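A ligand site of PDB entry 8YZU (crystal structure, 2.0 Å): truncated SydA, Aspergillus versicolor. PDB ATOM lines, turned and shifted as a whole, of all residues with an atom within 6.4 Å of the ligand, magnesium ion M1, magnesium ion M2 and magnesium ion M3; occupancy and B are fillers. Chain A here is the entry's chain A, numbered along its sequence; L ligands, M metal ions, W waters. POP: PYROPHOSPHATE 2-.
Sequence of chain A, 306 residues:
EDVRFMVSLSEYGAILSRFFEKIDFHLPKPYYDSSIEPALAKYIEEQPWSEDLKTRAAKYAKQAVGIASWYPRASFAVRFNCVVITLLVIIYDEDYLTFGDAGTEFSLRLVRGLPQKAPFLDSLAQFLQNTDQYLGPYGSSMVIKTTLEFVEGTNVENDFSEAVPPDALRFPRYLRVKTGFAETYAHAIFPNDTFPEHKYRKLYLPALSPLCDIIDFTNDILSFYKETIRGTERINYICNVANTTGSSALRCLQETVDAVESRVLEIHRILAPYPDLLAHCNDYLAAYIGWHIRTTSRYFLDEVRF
An oxygen (O6) of the ligand lies within salt-bridge range of the guanidinium group of Arg 298 (2.9 Å). An oxygen (O3) of the ligand lies within salt-bridge range of the guanidinium group (NH1) of Arg 176, 2.8 Å away. An oxygen (O5) of the ligand sits close to the side-chain amino group (NZ) of Lys 226 (2.8 Å). An oxygen (O6) of the ligand lies within hydrogen-bond range of the side-chain hydroxyl of Tyr 299 (2.4 Å).
The side-chain hydroxyl (OH) of Tyr 299 sits at hydrogen-bond distance from the guanidinium group (NE) of Arg 298. The side-chain carboxylate (OE1) of Glu 227 sits at hydrogen-bond distance from the side-chain amide nitrogen (ND2) of Asn 236, at 2.8 Å. OD2 of Asp 93 sits close to NH2 of Arg 298 (3.2 Å). The side-chain amide nitrogen (ND2) of Asn 219 is in hydrogen-bond range of a ring nitrogen (NE2) of His 292 (2.9 Å). The guanidinium group of Arg 176 sits close to the side-chain amide oxygen of Asn 219 (3.0 Å). NZ of Lys 226 lies close to OE2 of Glu 227. The guanidinium group of Arg 298 is in salt-bridge range of the side-chain carboxylate of Glu 94 (2.8 Å). OD2 of Asp 220 lies within salt-bridge range of NE of Arg 176 (2.9 Å).
Thr 179 touches the ligand. Within 4 Å of the ligand: Asp 93, Arg 176, Thr 179, Asn 219, Ser 223, Lys 226, Glu 227, Arg 298 and Tyr 299.
Merely in contact with magnesium ion M1: Glu 157 (3.97 Å). Within 4 Å of magnesium ion M1: Asp 93 and Glu 157. Along chain A the residues within 4 Å of magnesium ion M1 span positions 93 to 157. The nearest printed residue that does not touch magnesium ion M1 is Thr 179 (4.3 Å).
Merely in contact with magnesium ion M2: Lys 226. Two residues have an atom within 4 Å of magnesium ion M2: Asp 93 and Lys 226.
Three residues have an atom within 4 Å of magnesium ion M3: Asn 219, Ser 223 and Glu 227.
Water W4 binds magnesium ion M1, 1.9 Å away. O2 of the ligand binds magnesium ion M1, 2.0 Å away. The side-chain carboxylate (OD1) of Asp 93 is bound to magnesium ion M1, 2.1 Å away. Magnesium ion M1 is bound by water W7, 2.1 Å away. Water W3 is bound to magnesium ion M1 (2.2 Å). Magnesium ion M1 is bound by water W2.
O2 of the ligand binds magnesium ion M2 (2.0 Å). Water W6 is bound to magnesium ion M2, at 2.0 Å. Water W2 is bound to magnesium ion M2, 2.1 Å away. Water W5 is bound to magnesium ion M2, at 2.1 Å. O5 of the ligand is bound to magnesium ion M2, 2.1 Å away. Magnesium ion M2 is bound by the side-chain carboxylate (OD2) of Asp 93 (2.1 Å).
Magnesium ion M3 is bound by the side-chain carboxylate of Glu 227 (2.0 Å), an oxygen (O4) of the ligand (2.0 Å), an oxygen (O1) of the ligand (2.0 Å), water W1 (2.1 Å), the side-chain amide oxygen of Asn 219 (2.2 Å) and the side-chain hydroxyl of Ser 223 (2.3 Å). Magnesium ion M3 has six donor atoms within binding distance.
Water W4 lies within hydrogen-bond range of O of Thr 179 (2.5 Å) and O3 of the ligand (2.8 Å). Water W3 lies within hydrogen-bond range of the side-chain hydroxyl of Thr 154 and the side-chain carboxylate of Glu 157. Water W6 bridges the side-chain carboxylate of Glu 233 (2.9 Å) and the side-chain amino group of Lys 226 (3.4 Å). Water W5 lies within hydrogen-bond range of the side-chain amino group of Lys 226 (3.1 Å) and the side-chain carboxylate of Glu 94 (3.5 Å). Water W1 lies within hydrogen-bond range of OD1 of Asp 220 (2.7 Å) and OE1 of Glu 227 (2.8 Å).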
ATOM      1  N   ILE A  90       9.417  20.772 -16.003  1.00  0.00           N
ATOM      2  CA  ILE A  90       8.197  21.515 -16.355  1.00  0.00           C
ATOM      3  C   ILE A  90       7.174  21.449 -15.220  1.00  0.00           C
ATOM      4  O   ILE A  90       6.534  22.450 -14.883  1.00  0.00           O
ATOM      5  CB  ILE A  90       7.605  20.979 -17.673  1.00  0.00           C
ATOM      6  CG1 ILE A  90       8.462  21.382 -18.858  1.00  0.00           C
ATOM      7  CG2 ILE A  90       6.201  21.554 -17.870  1.00  0.00           C
ATOM      8  CD1 ILE A  90       8.038  20.704 -20.154  1.00  0.00           C
ATOM      9  N   ASP A  93       8.599  23.924 -12.640  1.00  0.00           N
ATOM     10  CA  ASP A  93       8.506  25.306 -13.135  1.00  0.00           C
ATOM     11  C   ASP A  93       7.083  25.847 -13.027  1.00  0.00           C
ATOM     12  O   ASP A  93       6.856  26.980 -12.568  1.00  0.00           O
ATOM     13  CB  ASP A  93       8.979  25.374 -14.587  1.00  0.00           C
ATOM     14  CG  ASP A  93       9.572  26.735 -14.957  1.00  0.00           C
ATOM     15  OD1 ASP A  93      10.575  27.145 -14.341  1.00  0.00           O
ATOM     16  OD2 ASP A  93       9.028  27.400 -15.859  1.00  0.00           O
ATOM     17  N   GLU A  94       6.102  25.040 -13.432  1.00  0.00           N
ATOM     18  CA  GLU A  94       4.707  25.460 -13.356  1.00  0.00           C
ATOM     19  C   GLU A  94       4.139  25.343 -11.939  1.00  0.00           C
ATOM     20  O   GLU A  94       3.439  26.244 -11.476  1.00  0.00           O
ATOM     21  CB  GLU A  94       3.880  24.628 -14.320  1.00  0.00           C
ATOM     22  CG  GLU A  94       4.351  24.699 -15.762  1.00  0.00           C
ATOM     23  CD  GLU A  94       4.319  26.128 -16.303  1.00  0.00           C
ATOM     24  OE1 GLU A  94       3.251  26.746 -16.216  1.00  0.00           O
ATOM     25  OE2 GLU A  94       5.381  26.628 -16.799  1.00  0.00           O
ATOM     26  N   PHE A 150      18.336  24.675  -9.759  1.00  0.00           N
ATOM     27  CA  PHE A 150      17.035  24.925 -10.368  1.00  0.00           C
ATOM     28  C   PHE A 150      15.918  24.900  -9.327  1.00  0.00           C
ATOM     29  O   PHE A 150      15.007  25.729  -9.382  1.00  0.00           O
ATOM     30  CB  PHE A 150      16.740  23.903 -11.470  1.00  0.00           C
ATOM     31  CG  PHE A 150      15.294  23.886 -11.897  1.00  0.00           C
ATOM     32  CD1 PHE A 150      14.820  24.835 -12.789  1.00  0.00           C
ATOM     33  CD2 PHE A 150      14.410  22.914 -11.415  1.00  0.00           C
ATOM     34  CE1 PHE A 150      13.484  24.842 -13.181  1.00  0.00           C
ATOM     35  CE2 PHE A 150      13.076  22.930 -11.809  1.00  0.00           C
ATOM     36  CZ  PHE A 150      12.616  23.884 -12.710  1.00  0.00           C
ATOM     37  N   THR A 154      13.930  28.449  -8.656  1.00  0.00           N
ATOM     38  CA  THR A 154      12.480  28.507  -8.841  1.00  0.00           C
ATOM     39  C   THR A 154      11.781  28.931  -7.551  1.00  0.00           C
ATOM     40  O   THR A 154      10.778  29.669  -7.595  1.00  0.00           O
ATOM     41  CB  THR A 154      11.967  27.140  -9.315  1.00  0.00           C
ATOM     42  OG1 THR A 154      12.586  26.800 -10.561  1.00  0.00           O
ATOM     43  CG2 THR A 154      10.393  27.103  -9.452  1.00  0.00           C
ATOM     44  N   GLU A 157      12.914  32.998  -7.014  1.00  0.00           N
ATOM     45  CA  GLU A 157      12.689  33.896  -8.151  1.00  0.00           C
ATOM     46  C   GLU A 157      11.782  35.090  -7.860  1.00  0.00           C
ATOM     47  O   GLU A 157      12.134  36.253  -8.119  1.00  0.00           O
ATOM     48  CB  GLU A 157      12.031  33.061  -9.251  1.00  0.00           C
ATOM     49  CG  GLU A 157      12.615  33.220 -10.572  1.00  0.00           C
ATOM     50  CD  GLU A 157      12.173  32.141 -11.504  1.00  0.00           C
ATOM     51  OE1 GLU A 157      11.508  31.155 -11.071  1.00  0.00           O
ATOM     52  OE2 GLU A 157      12.476  32.308 -12.699  1.00  0.00           O
ATOM     53  N   ARG A 176      19.796  33.774 -13.545  1.00  0.00           N
ATOM     54  CA  ARG A 176      19.495  32.958 -14.722  1.00  0.00           C
ATOM     55  C   ARG A 176      20.293  31.648 -14.743  1.00  0.00           C
ATOM     56  O   ARG A 176      19.784  30.628 -15.227  1.00  0.00           O
ATOM     57  CB  ARG A 176      19.742  33.733 -15.998  1.00  0.00           C
ATOM     58  CG  ARG A 176      19.285  32.963 -17.229  1.00  0.00           C
ATOM     59  CD  ARG A 176      17.872  32.378 -17.029  1.00  0.00           C
ATOM     60  NE  ARG A 176      17.273  31.945 -18.284  1.00  0.00           N
ATOM     61  CZ  ARG A 176      16.202  31.165 -18.385  1.00  0.00           C
ATOM     62  NH1 ARG A 176      15.618  30.623 -17.308  1.00  0.00           N
ATOM     63  NH2 ARG A 176      15.700  30.909 -19.602  1.00  0.00           N
ATOM     64  N   THR A 179      18.091  29.493 -12.508  1.00  0.00           N
ATOM     65  CA  THR A 179      16.772  29.082 -12.981  1.00  0.00           C
ATOM     66  C   THR A 179      16.823  28.329 -14.314  1.00  0.00           C
ATOM     67  O   THR A 179      15.845  27.635 -14.646  1.00  0.00           O
ATOM     68  CB  THR A 179      15.823  30.282 -13.157  1.00  0.00           C
ATOM     69  OG1 THR A 179      16.291  31.122 -14.220  1.00  0.00           O
ATOM     70  CG2 THR A 179      15.724  31.108 -11.877  1.00  0.00           C
ATOM     71  N   GLY A 180      17.910  28.459 -15.063  1.00  0.00           N
ATOM     72  CA  GLY A 180      17.913  28.003 -16.442  1.00  0.00           C
ATOM     73  C   GLY A 180      18.030  26.508 -16.684  1.00  0.00           C
ATOM     74  O   GLY A 180      17.588  26.019 -17.722  1.00  0.00           O
ATOM     75  N   PHE A 181      18.687  25.772 -15.781  1.00  0.00           N
ATOM     76  CA  PHE A 181      18.841  24.313 -15.931  1.00  0.00           C
ATOM     77  C   PHE A 181      19.696  23.922 -17.148  1.00  0.00           C
ATOM     78  O   PHE A 181      19.600  22.807 -17.642  1.00  0.00           O
ATOM     79  CB  PHE A 181      17.458  23.626 -16.012  1.00  0.00           C
ATOM     80  CG  PHE A 181      17.464  22.183 -15.631  1.00  0.00           C
ATOM     81  CD1 PHE A 181      17.722  21.799 -14.328  1.00  0.00           C
ATOM     82  CD2 PHE A 181      17.191  21.208 -16.574  1.00  0.00           C
ATOM     83  CE1 PHE A 181      17.732  20.453 -13.976  1.00  0.00           C
ATOM     84  CE2 PHE A 181      17.170  19.858 -16.227  1.00  0.00           C
ATOM     85  CZ  PHE A 181      17.451  19.490 -14.923  1.00  0.00           C
ATOM     86  N   ASN A 219      16.020  30.694 -24.737  1.00  0.00           N
ATOM     87  CA  ASN A 219      14.700  30.611 -24.110  1.00  0.00           C
ATOM     88  C   ASN A 219      14.246  31.979 -23.659  1.00  0.00           C
ATOM     89  O   ASN A 219      13.057  32.312 -23.763  1.00  0.00           O
ATOM     90  CB  ASN A 219      14.701  29.645 -22.921  1.00  0.00           C
ATOM     91  CG  ASN A 219      13.390  29.681 -22.158  1.00  0.00           C
ATOM     92  OD1 ASN A 219      13.238  30.430 -21.184  1.00  0.00           O
ATOM     93  ND2 ASN A 219      12.418  28.899 -22.622  1.00  0.00           N
ATOM     94  N   ASP A 220      15.149  32.780 -23.108  1.00  0.00           N
ATOM     95  CA  ASP A 220      14.769  34.136 -22.714  1.00  0.00           C
ATOM     96  C   ASP A 220      14.221  34.908 -23.905  1.00  0.00           C
ATOM     97  O   ASP A 220      13.145  35.525 -23.830  1.00  0.00           O
ATOM     98  CB  ASP A 220      15.954  34.838 -22.069  1.00  0.00           C
ATOM     99  CG  ASP A 220      16.229  34.312 -20.643  1.00  0.00           C
ATOM    100  OD1 ASP A 220      15.234  34.157 -19.901  1.00  0.00           O
ATOM    101  OD2 ASP A 220      17.409  34.050 -20.277  1.00  0.00           O
ATOM    102  N   SER A 223      10.811  33.003 -25.089  1.00  0.00           N
ATOM    103  CA  SER A 223       9.726  32.875 -24.128  1.00  0.00           C
ATOM    104  C   SER A 223       9.342  34.226 -23.552  1.00  0.00           C
ATOM    105  O   SER A 223       8.459  34.279 -22.683  1.00  0.00           O
ATOM    106  CB  SER A 223      10.073  31.891 -23.005  1.00  0.00           C
ATOM    107  OG  SER A 223      11.163  32.338 -22.204  1.00  0.00           O
ATOM    108  N   PHE A 224       9.973  35.305 -24.031  1.00  0.00           N
ATOM    109  CA  PHE A 224       9.589  36.642 -23.589  1.00  0.00           C
ATOM    110  C   PHE A 224       8.146  36.961 -23.949  1.00  0.00           C
ATOM    111  O   PHE A 224       7.495  37.697 -23.213  1.00  0.00           O
ATOM    112  CB  PHE A 224      10.538  37.695 -24.191  1.00  0.00           C
ATOM    113  CG  PHE A 224      10.277  39.076 -23.665  1.00  0.00           C
ATOM    114  CD1 PHE A 224      10.779  39.463 -22.435  1.00  0.00           C
ATOM    115  CD2 PHE A 224       9.503  39.984 -24.388  1.00  0.00           C
ATOM    116  CE1 PHE A 224      10.535  40.740 -21.928  1.00  0.00           C
ATOM    117  CE2 PHE A 224       9.259  41.261 -23.880  1.00  0.00           C
ATOM    118  CZ  PHE A 224       9.770  41.634 -22.655  1.00  0.00           C
ATOM    119  N   LYS A 226       5.475  34.758 -24.020  1.00  0.00           N
ATOM    120  CA  LYS A 226       4.521  34.136 -23.116  1.00  0.00           C
ATOM    121  C   LYS A 226       4.694  34.645 -21.688  1.00  0.00           C
ATOM    122  O   LYS A 226       3.726  34.671 -20.921  1.00  0.00           O
ATOM    123  CB  LYS A 226       4.634  32.599 -23.154  1.00  0.00           C
ATOM    124  CG  LYS A 226       5.913  32.043 -22.518  1.00  0.00           C
ATOM    125  CD  LYS A 226       5.663  31.457 -21.131  1.00  0.00           C
ATOM    126  CE  LYS A 226       6.809  30.568 -20.631  1.00  0.00           C
ATOM    127  NZ  LYS A 226       6.692  30.444 -19.138  1.00  0.00           N
ATOM    128  N   GLU A 227       5.899  35.065 -21.334  1.00  0.00           N
ATOM    129  CA  GLU A 227       6.210  35.501 -19.974  1.00  0.00           C
ATOM    130  C   GLU A 227       5.775  36.942 -19.713  1.00  0.00           C
ATOM    131  O   GLU A 227       5.156  37.226 -18.684  1.00  0.00           O
ATOM    132  CB  GLU A 227       7.714  35.335 -19.704  1.00  0.00           C
ATOM    133  CG  GLU A 227       8.146  33.878 -19.621  1.00  0.00           C
ATOM    134  CD  GLU A 227       9.643  33.668 -19.529  1.00  0.00           C
ATOM    135  OE1 GLU A 227      10.422  34.656 -19.442  1.00  0.00           O
ATOM    136  OE2 GLU A 227      10.031  32.475 -19.536  1.00  0.00           O
ATOM    137  N   GLU A 233       4.957  37.914 -15.988  1.00  0.00           N
ATOM    138  CA  GLU A 233       6.251  37.660 -15.358  1.00  0.00           C
ATOM    139  C   GLU A 233       7.200  38.822 -15.621  1.00  0.00           C
ATOM    140  O   GLU A 233       7.500  39.137 -16.777  1.00  0.00           O
ATOM    141  CB  GLU A 233       6.839  36.358 -15.878  1.00  0.00           C
ATOM    142  CG  GLU A 233       8.217  36.051 -15.332  1.00  0.00           C
ATOM    143  CD  GLU A 233       8.702  34.663 -15.708  1.00  0.00           C
ATOM    144  OE1 GLU A 233       7.857  33.790 -15.992  1.00  0.00           O
ATOM    145  OE2 GLU A 233       9.930  34.438 -15.683  1.00  0.00           O
ATOM    146  N   ASN A 236      11.923  37.641 -14.910  1.00  0.00           N
ATOM    147  CA  ASN A 236      12.803  36.873 -15.794  1.00  0.00           C
ATOM    148  C   ASN A 236      14.073  37.666 -16.107  1.00  0.00           C
ATOM    149  O   ASN A 236      14.225  38.848 -15.750  1.00  0.00           O
ATOM    150  CB  ASN A 236      12.062  36.479 -17.078  1.00  0.00           C
ATOM    151  CG  ASN A 236      11.394  37.653 -17.777  1.00  0.00           C
ATOM    152  OD1 ASN A 236      11.685  38.813 -17.494  1.00  0.00           O
ATOM    153  ND2 ASN A 236      10.474  37.345 -18.695  1.00  0.00           N
ATOM    154  N   TRP A 291      11.407  23.496 -31.315  1.00  0.00           N
ATOM    155  CA  TRP A 291      10.517  23.052 -30.240  1.00  0.00           C
ATOM    156  C   TRP A 291       9.821  24.237 -29.577  1.00  0.00           C
ATOM    157  O   TRP A 291       8.646  24.147 -29.208  1.00  0.00           O
ATOM    158  CB  TRP A 291      11.298  22.217 -29.231  1.00  0.00           C
ATOM    159  CG  TRP A 291      10.488  21.793 -28.041  1.00  0.00           C
ATOM    160  CD1 TRP A 291       9.665  20.694 -27.944  1.00  0.00           C
ATOM    161  CD2 TRP A 291      10.413  22.451 -26.770  1.00  0.00           C
ATOM    162  NE1 TRP A 291       9.104  20.629 -26.690  1.00  0.00           N
ATOM    163  CE2 TRP A 291       9.551  21.709 -25.949  1.00  0.00           C
ATOM    164  CE3 TRP A 291      11.020  23.605 -26.244  1.00  0.00           C
ATOM    165  CZ2 TRP A 291       9.245  22.073 -24.641  1.00  0.00           C
ATOM    166  CZ3 TRP A 291      10.726  23.977 -24.936  1.00  0.00           C
ATOM    167  CH2 TRP A 291       9.858  23.207 -24.151  1.00  0.00           C
ATOM    168  N   HIS A 292      10.536  25.351 -29.391  1.00  0.00           N
ATOM    169  CA  HIS A 292       9.907  26.560 -28.861  1.00  0.00           C
ATOM    170  C   HIS A 292       8.815  27.056 -29.793  1.00  0.00           C
ATOM    171  O   HIS A 292       7.738  27.485 -29.341  1.00  0.00           O
ATOM    172  CB  HIS A 292      10.968  27.659 -28.648  1.00  0.00           C
ATOM    173  CG  HIS A 292      11.700  27.584 -27.339  1.00  0.00           C
ATOM    174  ND1 HIS A 292      12.823  26.793 -27.139  1.00  0.00           N
ATOM    175  CD2 HIS A 292      11.496  28.218 -26.158  1.00  0.00           C
ATOM    176  CE1 HIS A 292      13.256  26.933 -25.899  1.00  0.00           C
ATOM    177  NE2 HIS A 292      12.458  27.792 -25.283  1.00  0.00           N
ATOM    178  N   ARG A 298       2.800  26.152 -24.888  1.00  0.00           N
ATOM    179  CA  ARG A 298       3.662  26.749 -23.857  1.00  0.00           C
ATOM    180  C   ARG A 298       4.138  28.161 -24.222  1.00  0.00           C
ATOM    181  O   ARG A 298       4.215  29.022 -23.334  1.00  0.00           O
ATOM    182  CB  ARG A 298       4.870  25.839 -23.583  1.00  0.00           C
ATOM    183  CG  ARG A 298       5.650  26.147 -22.266  1.00  0.00           C
ATOM    184  CD  ARG A 298       6.765  25.135 -21.904  1.00  0.00           C
ATOM    185  NE  ARG A 298       7.469  25.560 -20.701  1.00  0.00           N
ATOM    186  CZ  ARG A 298       6.920  25.608 -19.490  1.00  0.00           C
ATOM    187  NH1 ARG A 298       5.705  25.107 -19.268  1.00  0.00           N
ATOM    188  NH2 ARG A 298       7.576  26.183 -18.491  1.00  0.00           N
ATOM    189  N   TYR A 299       4.485  28.415 -25.489  1.00  0.00           N
ATOM    190  CA  TYR A 299       5.121  29.684 -25.844  1.00  0.00           C
ATOM    191  C   TYR A 299       4.285  30.567 -26.762  1.00  0.00           C
ATOM    192  O   TYR A 299       4.589  31.767 -26.882  1.00  0.00           O
ATOM    193  CB  TYR A 299       6.516  29.439 -26.473  1.00  0.00           C
ATOM    194  CG  TYR A 299       7.427  28.688 -25.507  1.00  0.00           C
ATOM    195  CD1 TYR A 299       7.925  29.316 -24.373  1.00  0.00           C
ATOM    196  CD2 TYR A 299       7.729  27.351 -25.698  1.00  0.00           C
ATOM    197  CE1 TYR A 299       8.713  28.637 -23.453  1.00  0.00           C
ATOM    198  CE2 TYR A 299       8.538  26.653 -24.789  1.00  0.00           C
ATOM    199  CZ  TYR A 299       9.021  27.304 -23.665  1.00  0.00           C
ATOM    200  OH  TYR A 299       9.811  26.610 -22.761  1.00  0.00           O
HETATM  201  P1  POP L   1      12.111  29.259 -17.858  1.00  0.00           P
HETATM  202  O1  POP L   1      12.103  30.704 -18.357  1.00  0.00           O
HETATM  203  O2  POP L   1      11.312  29.159 -16.554  1.00  0.00           O
HETATM  204  O3  POP L   1      13.516  28.777 -17.551  1.00  0.00           O
HETATM  205  O   POP L   1      11.456  28.288 -18.948  1.00  0.00           O
HETATM  206  P2  POP L   1      10.082  28.652 -19.681  1.00  0.00           P
HETATM  207  O4  POP L   1      10.386  29.815 -20.597  1.00  0.00           O
HETATM  208  O5  POP L   1       9.002  29.011 -18.677  1.00  0.00           O
HETATM  209  O6  POP L   1       9.646  27.435 -20.484  1.00  0.00           O
HETATM  210 MG    MG M   1      11.764  28.889 -14.589  1.00  0.00          MG
HETATM  211 MG    MG M   2       9.346  29.354 -16.623  1.00  0.00          MG
HETATM  212 MG    MG M   3      11.555  31.389 -20.169  1.00  0.00          MG
HETATM  213  O   HOH W   1      12.733  33.129 -20.036  1.00  0.00           O
HETATM  214  O   HOH W   2       9.743  29.928 -14.694  1.00  0.00           O
HETATM  215  O   HOH W   3      12.114  28.726 -12.432  1.00  0.00           O
HETATM  216  O   HOH W   4      13.381  27.988 -14.911  1.00  0.00           O
HETATM  217  O   HOH W   5       7.287  29.504 -16.260  1.00  0.00           O
HETATM  218  O   HOH W   6       9.077  31.314 -16.946  1.00  0.00           O
HETATM  219  O   HOH W   7      12.639  30.827 -14.435  1.00  0.00           O
HETATM  220  O   HOH W   8      12.405  32.717 -16.622  1.00  0.00           O
